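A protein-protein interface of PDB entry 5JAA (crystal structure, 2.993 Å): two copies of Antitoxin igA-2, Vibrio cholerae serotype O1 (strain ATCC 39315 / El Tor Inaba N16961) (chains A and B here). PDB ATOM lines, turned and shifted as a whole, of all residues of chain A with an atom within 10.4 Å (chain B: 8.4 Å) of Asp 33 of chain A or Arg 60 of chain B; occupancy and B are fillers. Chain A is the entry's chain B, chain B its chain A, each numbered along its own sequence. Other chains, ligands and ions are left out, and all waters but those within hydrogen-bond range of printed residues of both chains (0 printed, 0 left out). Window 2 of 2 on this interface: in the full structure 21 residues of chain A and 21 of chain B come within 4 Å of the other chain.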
ATOM      1  N   HIS A  30      21.641 -13.699  18.662  1.00  0.00           N
ATOM      2  CA  HIS A  30      22.815 -14.184  17.947  1.00  0.00           C
ATOM      3  C   HIS A  30      22.695 -13.828  16.469  1.00  0.00           C
ATOM      4  O   HIS A  30      21.754 -14.250  15.799  1.00  0.00           O
ATOM      5  CB  HIS A  30      22.969 -15.699  18.106  1.00  0.00           C
ATOM      6  CG  HIS A  30      23.146 -16.150  19.523  1.00  0.00           C
ATOM      7  ND1 HIS A  30      24.104 -15.621  20.362  1.00  0.00           N
ATOM      8  CD2 HIS A  30      22.498 -17.098  20.243  1.00  0.00           C
ATOM      9  CE1 HIS A  30      24.031 -16.215  21.540  1.00  0.00           C
ATOM     10  NE2 HIS A  30      23.066 -17.115  21.494  1.00  0.00           N
ATOM     11  N   VAL A  31      23.647 -13.052  15.965  1.00  0.00           N
ATOM     12  CA  VAL A  31      23.621 -12.624  14.571  1.00  0.00           C
ATOM     13  C   VAL A  31      24.948 -12.930  13.872  1.00  0.00           C
ATOM     14  O   VAL A  31      26.019 -12.658  14.408  1.00  0.00           O
ATOM     15  CB  VAL A  31      23.303 -11.116  14.463  1.00  0.00           C
ATOM     16  CG1 VAL A  31      23.565 -10.602  13.057  1.00  0.00           C
ATOM     17  CG2 VAL A  31      21.860 -10.849  14.879  1.00  0.00           C
ATOM     18  N   ASN A  32      24.865 -13.511  12.678  1.00  0.00           N
ATOM     19  CA  ASN A  32      26.053 -13.839  11.894  1.00  0.00           C
ATOM     20  C   ASN A  32      26.033 -13.163  10.526  1.00  0.00           C
ATOM     21  O   ASN A  32      24.986 -12.715  10.060  1.00  0.00           O
ATOM     22  CB  ASN A  32      26.186 -15.354  11.737  1.00  0.00           C
ATOM     23  CG  ASN A  32      24.846 -16.041  11.620  1.00  0.00           C
ATOM     24  OD1 ASN A  32      23.861 -15.434  11.203  1.00  0.00           O
ATOM     25  ND2 ASN A  32      24.797 -17.312  11.999  1.00  0.00           N
ATOM     26  N   ASP A  33      27.201 -13.085   9.893  1.00  0.00           N
ATOM     27  CA  ASP A  33      27.371 -12.328   8.654  1.00  0.00           C
ATOM     28  C   ASP A  33      26.877 -13.093   7.428  1.00  0.00           C
ATOM     29  O   ASP A  33      26.400 -14.223   7.537  1.00  0.00           O
ATOM     30  CB  ASP A  33      28.844 -11.950   8.472  1.00  0.00           C
ATOM     31  CG  ASP A  33      29.035 -10.715   7.609  1.00  0.00           C
ATOM     32  OD1 ASP A  33      28.185 -10.456   6.730  1.00  0.00           O
ATOM     33  OD2 ASP A  33      30.042 -10.003   7.809  1.00  0.00           O
ATOM     34  N   VAL A  34      26.991 -12.461   6.262  1.00  0.00           N
ATOM     35  CA  VAL A  34      26.620 -13.082   4.998  1.00  0.00           C
ATOM     36  C   VAL A  34      27.708 -14.045   4.539  1.00  0.00           C
ATOM     37  O   VAL A  34      27.459 -14.943   3.734  1.00  0.00           O
ATOM     38  CB  VAL A  34      26.381 -12.033   3.894  1.00  0.00           C
ATOM     39  CG1 VAL A  34      25.274 -11.074   4.296  1.00  0.00           C
ATOM     40  CG2 VAL A  34      27.666 -11.277   3.595  1.00  0.00           C
ATOM     41  N   GLY A  35      28.917 -13.845   5.057  1.00  0.00           N
ATOM     42  CA  GLY A  35      30.053 -14.664   4.689  1.00  0.00           C
ATOM     43  C   GLY A  35      30.412 -14.536   3.223  1.00  0.00           C
ATOM     44  O   GLY A  35      30.215 -13.487   2.610  1.00  0.00           O
ATOM     45  N   GLU A  36      30.949 -15.615   2.667  1.00  0.00           N
ATOM     46  CA  GLU A  36      31.345 -15.653   1.265  1.00  0.00           C
ATOM     47  C   GLU A  36      30.539 -16.705   0.510  1.00  0.00           C
ATOM     48  O   GLU A  36      30.084 -17.689   1.095  1.00  0.00           O
ATOM     49  CB  GLU A  36      32.843 -15.940   1.136  1.00  0.00           C
ATOM     50  N   LEU A  37      30.363 -16.491  -0.788  1.00  0.00           N
ATOM     51  CA  LEU A  37      29.623 -17.426  -1.624  1.00  0.00           C
ATOM     52  C   LEU A  37      30.553 -18.131  -2.603  1.00  0.00           C
ATOM     53  O   LEU A  37      31.587 -17.587  -2.994  1.00  0.00           O
ATOM     54  CB  LEU A  37      28.514 -16.706  -2.389  1.00  0.00           C
ATOM     55  CG  LEU A  37      27.430 -16.007  -1.570  1.00  0.00           C
ATOM     56  CD1 LEU A  37      26.462 -15.285  -2.494  1.00  0.00           C
ATOM     57  CD2 LEU A  37      26.695 -17.001  -0.681  1.00  0.00           C
ATOM     58  N   GLY A  81      32.880 -11.629  -7.509  1.00  0.00           N
ATOM     59  CA  GLY A  81      31.916 -11.639  -6.424  1.00  0.00           C
ATOM     60  C   GLY A  81      30.488 -11.405  -6.870  1.00  0.00           C
ATOM     61  O   GLY A  81      29.587 -12.191  -6.560  1.00  0.00           O
ATOM     62  N   GLN A  82      30.278 -10.323  -7.609  1.00  0.00           N
ATOM     63  CA  GLN A  82      28.942  -9.963  -8.054  1.00  0.00           C
ATOM     64  C   GLN A  82      28.419 -11.006  -9.030  1.00  0.00           C
ATOM     65  O   GLN A  82      27.214 -11.239  -9.117  1.00  0.00           O
ATOM     66  CB  GLN A  82      28.941  -8.573  -8.689  1.00  0.00           C
ATOM     67  CG  GLN A  82      29.301  -7.449  -7.724  1.00  0.00           C
ATOM     68  CD  GLN A  82      30.785  -7.370  -7.442  1.00  0.00           C
ATOM     69  OE1 GLN A  82      31.609  -7.562  -8.335  1.00  0.00           O
ATOM     70  NE2 GLN A  82      31.136  -7.095  -6.191  1.00  0.00           N
ATOM     71  N   THR A  85      27.257 -13.911  -6.886  1.00  0.00           N
ATOM     72  CA  THR A  85      26.041 -13.424  -6.246  1.00  0.00           C
ATOM     73  C   THR A  85      24.853 -13.532  -7.185  1.00  0.00           C
ATOM     74  O   THR A  85      23.807 -14.080  -6.838  1.00  0.00           O
ATOM     75  CB  THR A  85      26.181 -11.958  -5.812  1.00  0.00           C
ATOM     76  OG1 THR A  85      27.399 -11.783  -5.078  1.00  0.00           O
ATOM     77  CG2 THR A  85      24.995 -11.539  -4.962  1.00  0.00           C
ATOM     78  N   MET B  53      21.199   2.751   4.214  1.00  0.00           N
ATOM     79  CA  MET B  53      22.362   1.939   4.556  1.00  0.00           C
ATOM     80  C   MET B  53      23.678   2.688   4.415  1.00  0.00           C
ATOM     81  O   MET B  53      23.833   3.551   3.549  1.00  0.00           O
ATOM     82  CB  MET B  53      22.416   0.695   3.682  1.00  0.00           C
ATOM     83  CG  MET B  53      21.333  -0.310   3.954  1.00  0.00           C
ATOM     84  SD  MET B  53      21.606  -1.879   2.846  1.00  0.00           S
ATOM     85  CE  MET B  53      20.229  -3.026   3.617  1.00  0.00           C
ATOM     86  N   SER B  54      24.626   2.338   5.275  1.00  0.00           N
ATOM     87  CA  SER B  54      25.987   2.829   5.163  1.00  0.00           C
ATOM     88  C   SER B  54      26.688   2.142   3.996  1.00  0.00           C
ATOM     89  O   SER B  54      26.232   1.099   3.516  1.00  0.00           O
ATOM     90  CB  SER B  54      26.757   2.590   6.462  1.00  0.00           C
ATOM     91  OG  SER B  54      26.917   1.204   6.713  1.00  0.00           O
ATOM     92  N   ARG B  55      27.783   2.741   3.535  1.00  0.00           N
ATOM     93  CA  ARG B  55      28.619   2.130   2.508  1.00  0.00           C
ATOM     94  C   ARG B  55      29.061   0.723   2.896  1.00  0.00           C
ATOM     95  O   ARG B  55      29.048  -0.175   2.066  1.00  0.00           O
ATOM     96  CB  ARG B  55      29.848   2.997   2.224  1.00  0.00           C
ATOM     97  CG  ARG B  55      29.583   4.151   1.280  1.00  0.00           C
ATOM     98  CD  ARG B  55      30.689   5.187   1.354  1.00  0.00           C
ATOM     99  NE  ARG B  55      30.487   6.250   0.376  1.00  0.00           N
ATOM    100  CZ  ARG B  55      31.215   7.359   0.315  1.00  0.00           C
ATOM    101  NH1 ARG B  55      32.195   7.559   1.185  1.00  0.00           N
ATOM    102  NH2 ARG B  55      30.958   8.271  -0.615  1.00  0.00           N
ATOM    103  N   GLY B  56      29.435   0.533   4.157  1.00  0.00           N
ATOM    104  CA  GLY B  56      29.940  -0.749   4.618  1.00  0.00           C
ATOM    105  C   GLY B  56      28.959  -1.904   4.500  1.00  0.00           C
ATOM    106  O   GLY B  56      29.278  -2.951   3.922  1.00  0.00           O
ATOM    107  N   VAL B  57      27.766  -1.720   5.057  1.00  0.00           N
ATOM    108  CA  VAL B  57      26.735  -2.752   5.038  1.00  0.00           C
ATOM    109  C   VAL B  57      26.335  -3.097   3.608  1.00  0.00           C
ATOM    110  O   VAL B  57      26.364  -4.263   3.197  1.00  0.00           O
ATOM    111  CB  VAL B  57      25.484  -2.309   5.819  1.00  0.00           C
ATOM    112  CG1 VAL B  57      24.419  -3.392   5.774  1.00  0.00           C
ATOM    113  CG2 VAL B  57      25.847  -1.964   7.258  1.00  0.00           C
ATOM    114  N   PHE B  58      25.978  -2.062   2.856  1.00  0.00           N
ATOM    115  CA  PHE B  58      25.577  -2.209   1.467  1.00  0.00           C
ATOM    116  C   PHE B  58      26.655  -2.911   0.643  1.00  0.00           C
ATOM    117  O   PHE B  58      26.351  -3.773  -0.183  1.00  0.00           O
ATOM    118  CB  PHE B  58      25.259  -0.841   0.866  1.00  0.00           C
ATOM    119  CG  PHE B  58      24.655  -0.910  -0.499  1.00  0.00           C
ATOM    120  CD1 PHE B  58      23.406  -1.473  -0.682  1.00  0.00           C
ATOM    121  CD2 PHE B  58      25.332  -0.413  -1.598  1.00  0.00           C
ATOM    122  CE1 PHE B  58      22.841  -1.541  -1.932  1.00  0.00           C
ATOM    123  CE2 PHE B  58      24.772  -0.477  -2.852  1.00  0.00           C
ATOM    124  CZ  PHE B  58      23.524  -1.043  -3.021  1.00  0.00           C
ATOM    125  N   ALA B  59      27.915  -2.547   0.880  1.00  0.00           N
ATOM    126  CA  ALA B  59      29.037  -3.154   0.168  1.00  0.00           C
ATOM    127  C   ALA B  59      29.179  -4.616   0.539  1.00  0.00           C
ATOM    128  O   ALA B  59      29.546  -5.443  -0.294  1.00  0.00           O
ATOM    129  CB  ALA B  59      30.327  -2.414   0.455  1.00  0.00           C
ATOM    130  N   ARG B  60      28.893  -4.932   1.798  1.00  0.00           N
ATOM    131  CA  ARG B  60      28.908  -6.319   2.235  1.00  0.00           C
ATOM    132  C   ARG B  60      27.846  -7.108   1.481  1.00  0.00           C
ATOM    133  O   ARG B  60      28.094  -8.226   1.035  1.00  0.00           O
ATOM    134  CB  ARG B  60      28.681  -6.422   3.742  1.00  0.00           C
ATOM    135  CG  ARG B  60      28.837  -7.830   4.277  1.00  0.00           C
ATOM    136  CD  ARG B  60      30.243  -8.339   4.015  1.00  0.00           C
ATOM    137  NE  ARG B  60      31.213  -7.755   4.935  1.00  0.00           N
ATOM    138  CZ  ARG B  60      31.840  -8.441   5.884  1.00  0.00           C
ATOM    139  NH1 ARG B  60      31.608  -9.739   6.028  1.00  0.00           N
ATOM    140  NH2 ARG B  60      32.707  -7.833   6.681  1.00  0.00           N
ATOM    141  N   LEU B  61      26.667  -6.511   1.328  1.00  0.00           N
ATOM    142  CA  LEU B  61      25.578  -7.153   0.598  1.00  0.00           C
ATOM    143  C   LEU B  61      25.938  -7.430  -0.858  1.00  0.00           C
ATOM    144  O   LEU B  61      25.510  -8.427  -1.429  1.00  0.00           O
ATOM    145  CB  LEU B  61      24.312  -6.300   0.660  1.00  0.00           C
ATOM    146  CG  LEU B  61      23.340  -6.639   1.789  1.00  0.00           C
ATOM    147  CD1 LEU B  61      23.072  -8.126   1.788  1.00  0.00           C
ATOM    148  CD2 LEU B  61      23.878  -6.197   3.138  1.00  0.00           C
ATOM    149  N   LEU B  62      26.739  -6.556  -1.451  1.00  0.00           N
ATOM    150  CA  LEU B  62      27.141  -6.726  -2.842  1.00  0.00           C
ATOM    151  C   LEU B  62      28.413  -7.560  -2.944  1.00  0.00           C
ATOM    152  O   LEU B  62      28.982  -7.709  -4.025  1.00  0.00           O
ATOM    153  CB  LEU B  62      27.341  -5.370  -3.512  1.00  0.00           C
ATOM    154  CG  LEU B  62      26.094  -4.488  -3.554  1.00  0.00           C
ATOM    155  CD1 LEU B  62      26.368  -3.220  -4.320  1.00  0.00           C
ATOM    156  CD2 LEU B  62      24.910  -5.244  -4.127  1.00  0.00           C
ATOM    157  N   HIS B  63      28.855  -8.078  -1.800  1.00  0.00           N
ATOM    158  CA  HIS B  63      30.050  -8.915  -1.704  1.00  0.00           C
ATOM    159  C   HIS B  63      31.262  -8.240  -2.338  1.00  0.00           C
ATOM    160  O   HIS B  63      31.950  -8.824  -3.177  1.00  0.00           O
ATOM    161  CB  HIS B  63      29.802 -10.288  -2.334  1.00  0.00           C
ATOM    162  CG  HIS B  63      28.878 -11.158  -1.534  1.00  0.00           C
ATOM    163  ND1 HIS B  63      27.507 -11.112  -1.667  1.00  0.00           N
ATOM    164  CD2 HIS B  63      29.130 -12.090  -0.583  1.00  0.00           C
ATOM    165  CE1 HIS B  63      26.954 -11.980  -0.839  1.00  0.00           C
ATOM    166  NE2 HIS B  63      27.918 -12.586  -0.168  1.00  0.00           N
ATOM    167  N   THR B  64      31.496  -6.997  -1.924  1.00  0.00           N
ATOM    168  CA  THR B  64      32.670  -6.225  -2.317  1.00  0.00           C
ATOM    169  C   THR B  64      33.114  -5.353  -1.140  1.00  0.00           C
ATOM    170  O   THR B  64      32.371  -5.184  -0.174  1.00  0.00           O
ATOM    171  CB  THR B  64      32.393  -5.338  -3.544  1.00  0.00           C
ATOM    172  OG1 THR B  64      33.614  -4.723  -3.980  1.00  0.00           O
ATOM    173  CG2 THR B  64      31.375  -4.259  -3.202  1.00  0.00           C
ATOM    174  N   SER B  65      34.323  -4.806  -1.219  1.00  0.00           N
ATOM    175  CA  SER B  65      34.855  -3.962  -0.152  1.00  0.00           C
ATOM    176  C   SER B  65      34.231  -2.566  -0.145  1.00  0.00           C
ATOM    177  O   SER B  65      33.800  -2.062  -1.180  1.00  0.00           O
ATOM    178  CB  SER B  65      36.376  -3.839  -0.275  1.00  0.00           C
ATOM    179  OG  SER B  65      36.736  -2.997  -1.355  1.00  0.00           O
ATOM    180  N   SER B  66      34.191  -1.949   1.033  1.00  0.00           N
ATOM    181  CA  SER B  66      33.684  -0.588   1.182  1.00  0.00           C
ATOM    182  C   SER B  66      34.492   0.382   0.340  1.00  0.00           C
ATOM    183  O   SER B  66      33.948   1.322  -0.241  1.00  0.00           O
ATOM    184  CB  SER B  66      33.725  -0.157   2.645  1.00  0.00           C
ATOM    185  OG  SER B  66      33.131  -1.137   3.475  1.00  0.00           O
ATOM    186  N   LEU B  69      33.277   0.129  -3.311  1.00  0.00           N
ATOM    187  CA  LEU B  69      31.992   0.802  -3.463  1.00  0.00           C
ATOM    188  C   LEU B  69      32.169   2.313  -3.455  1.00  0.00           C
ATOM    189  O   LEU B  69      31.596   3.012  -4.287  1.00  0.00           O
ATOM    190  CB  LEU B  69      31.022   0.382  -2.356  1.00  0.00           C
ATOM    191  CG  LEU B  69      29.675   1.111  -2.333  1.00  0.00           C
ATOM    192  CD1 LEU B  69      28.887   0.850  -3.610  1.00  0.00           C
ATOM    193  CD2 LEU B  69      28.863   0.707  -1.117  1.00  0.00           C
ATOM    194  N   LEU B  97      17.239  -7.374  -2.627  1.00  0.00           N
ATOM    195  CA  LEU B  97      18.333  -7.156  -1.683  1.00  0.00           C
ATOM    196  C   LEU B  97      18.178  -8.068  -0.467  1.00  0.00           C
ATOM    197  O   LEU B  97      19.167  -8.534   0.111  1.00  0.00           O
ATOM    198  CB  LEU B  97      18.395  -5.690  -1.252  1.00  0.00           C
ATOM    199  CG  LEU B  97      19.606  -5.255  -0.420  1.00  0.00           C
ATOM    200  CD1 LEU B  97      20.908  -5.463  -1.174  1.00  0.00           C
ATOM    201  CD2 LEU B  97      19.467  -3.802  -0.006  1.00  0.00           C
ATOM    202  N   ILE B 100      19.327 -11.507  -1.678  1.00  0.00           N
ATOM    203  CA  ILE B 100      20.783 -11.492  -1.607  1.00  0.00           C
ATOM    204  C   ILE B 100      21.275 -11.678  -0.174  1.00  0.00           C
ATOM    205  O   ILE B 100      22.210 -12.440   0.074  1.00  0.00           O
ATOM    206  CB  ILE B 100      21.353 -10.174  -2.173  1.00  0.00           C
ATOM    207  CG1 ILE B 100      21.083 -10.080  -3.677  1.00  0.00           C
ATOM    208  CG2 ILE B 100      22.836 -10.070  -1.895  1.00  0.00           C
ATOM    209  CD1 ILE B 100      21.711  -8.873  -4.341  1.00  0.00           C
ATOM    210  N   ALA B 101      20.636 -10.983   0.764  1.00  0.00           N
ATOM    211  CA  ALA B 101      21.027 -11.047   2.171  1.00  0.00           C
ATOM    212  C   ALA B 101      20.948 -12.459   2.753  1.00  0.00           C
ATOM    213  O   ALA B 101      21.867 -12.905   3.437  1.00  0.00           O
ATOM    214  CB  ALA B 101      20.169 -10.102   2.987  1.00  0.00           C
ATOM    215  N   GLU B 102      19.851 -13.158   2.475  1.00  0.00           N
ATOM    216  CA  GLU B 102      19.611 -14.479   3.051  1.00  0.00           C
ATOM    217  C   GLU B 102      20.177 -15.592   2.178  1.00  0.00           C
ATOM    218  O   GLU B 102      19.985 -16.773   2.461  1.00  0.00           O
ATOM    219  CB  GLU B 102      18.111 -14.704   3.270  1.00  0.00           C
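Hydrophobic or aromatic side chains of chain B that line the printed part of chain A: His 63. Along chain B the printed residues that touch a printed residue of chain A span positions 60 to 101. Hydrophobic or aromatic side chains of chain A within 4 Å of the printed part of chain B: Val 34 and Leu 37. Among the printed residues, Asp or Glu carboxylates within 4 Å of a Lys or Arg side-chain nitrogen of the other chain: Asp 33 of chain A with Arg 60 of chain B.
N of Thr 64 of chain B lies within hydrogen-bond range of O of Ala 59 of chain B, at 3.0 Å. The side-chain hydroxyl (OG1) of Thr 85 of chain A lies within hydrogen-bond range of the backbone carbonyl oxygen (O) of Gly 81 of chain A (2.7 Å). O of Leu 61 of chain B sits at hydrogen-bond distance from ND1 of His 63 of chain B, 3.4 Å away.
No position is printed for both chains. Of the 10 pairs that touch across the chains among the printed residues, none has its exchanged pair printed and touching as well.
Val 34 of chain A touches Arg 60 of chain B (CG2 to CG, 3.7 Å). CG2 of Val 34 of chain A touches NE2 of His 63 of chain B, at 3.99 Å. Val 34 of chain A touches Ala 101 of chain B. Gly 35 of chain A touches His 63 of chain B. His 63 of chain B touches Leu 37 of chain A (CE1 to CD1, 3.7 Å). Gln 82 of chain A touches His 63 of chain B (NE2 to O, 3.6 Å). CB of Thr 64 of chain B touches NE2 of Gln 82 of chain A, at 3.4 Å.
Of chain A, only Asp 33 (2.4 Å) and Val 34 (3.7 Å) come within 4 Å of Arg 60 of chain B. No residue of chain A comes within 4 Å of Gly 56 of chain B. No residue of chain A comes within 4 Å of Val 57 of chain B. No residue of chain A comes within 4 Å of Ala 59 of chain B. No residue of chain A comes within 4 Å of Leu 61 of chain B. Of the printed residues of chain B, Leu 37 of chain A touches His 63. Printed residues of chain A within 4 Å of Ala 101 of chain B: Val 34 (3.96 Å). Ser 65 of chain B touches none of the printed residues of chain A. Met 53 of chain B touches none of the printed residues of chain A. The nearest residue of chain A that does not touch Arg 60 of chain B is Gly 35 of chain A (5.0 Å). The nearest printed residue of chain A that does not touch Thr 64 of chain B is Gly 81 of chain A (6.5 Å).
The guanidinium group (NH1) of Arg 60 of chain B is in salt-bridge range of the side-chain carboxylate (OD1) of Asp 33 of chain A (3.6 Å). The side-chain amide nitrogen (NE2) of Gln 82 of chain A sits at hydrogen-bond distance from the backbone carbonyl oxygen (O) of Leu 62 of chain B. ND1 of His 63 of chain B sits at hydrogen-bond distance from OG1 of Thr 85 of chain A (3.5 Å).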
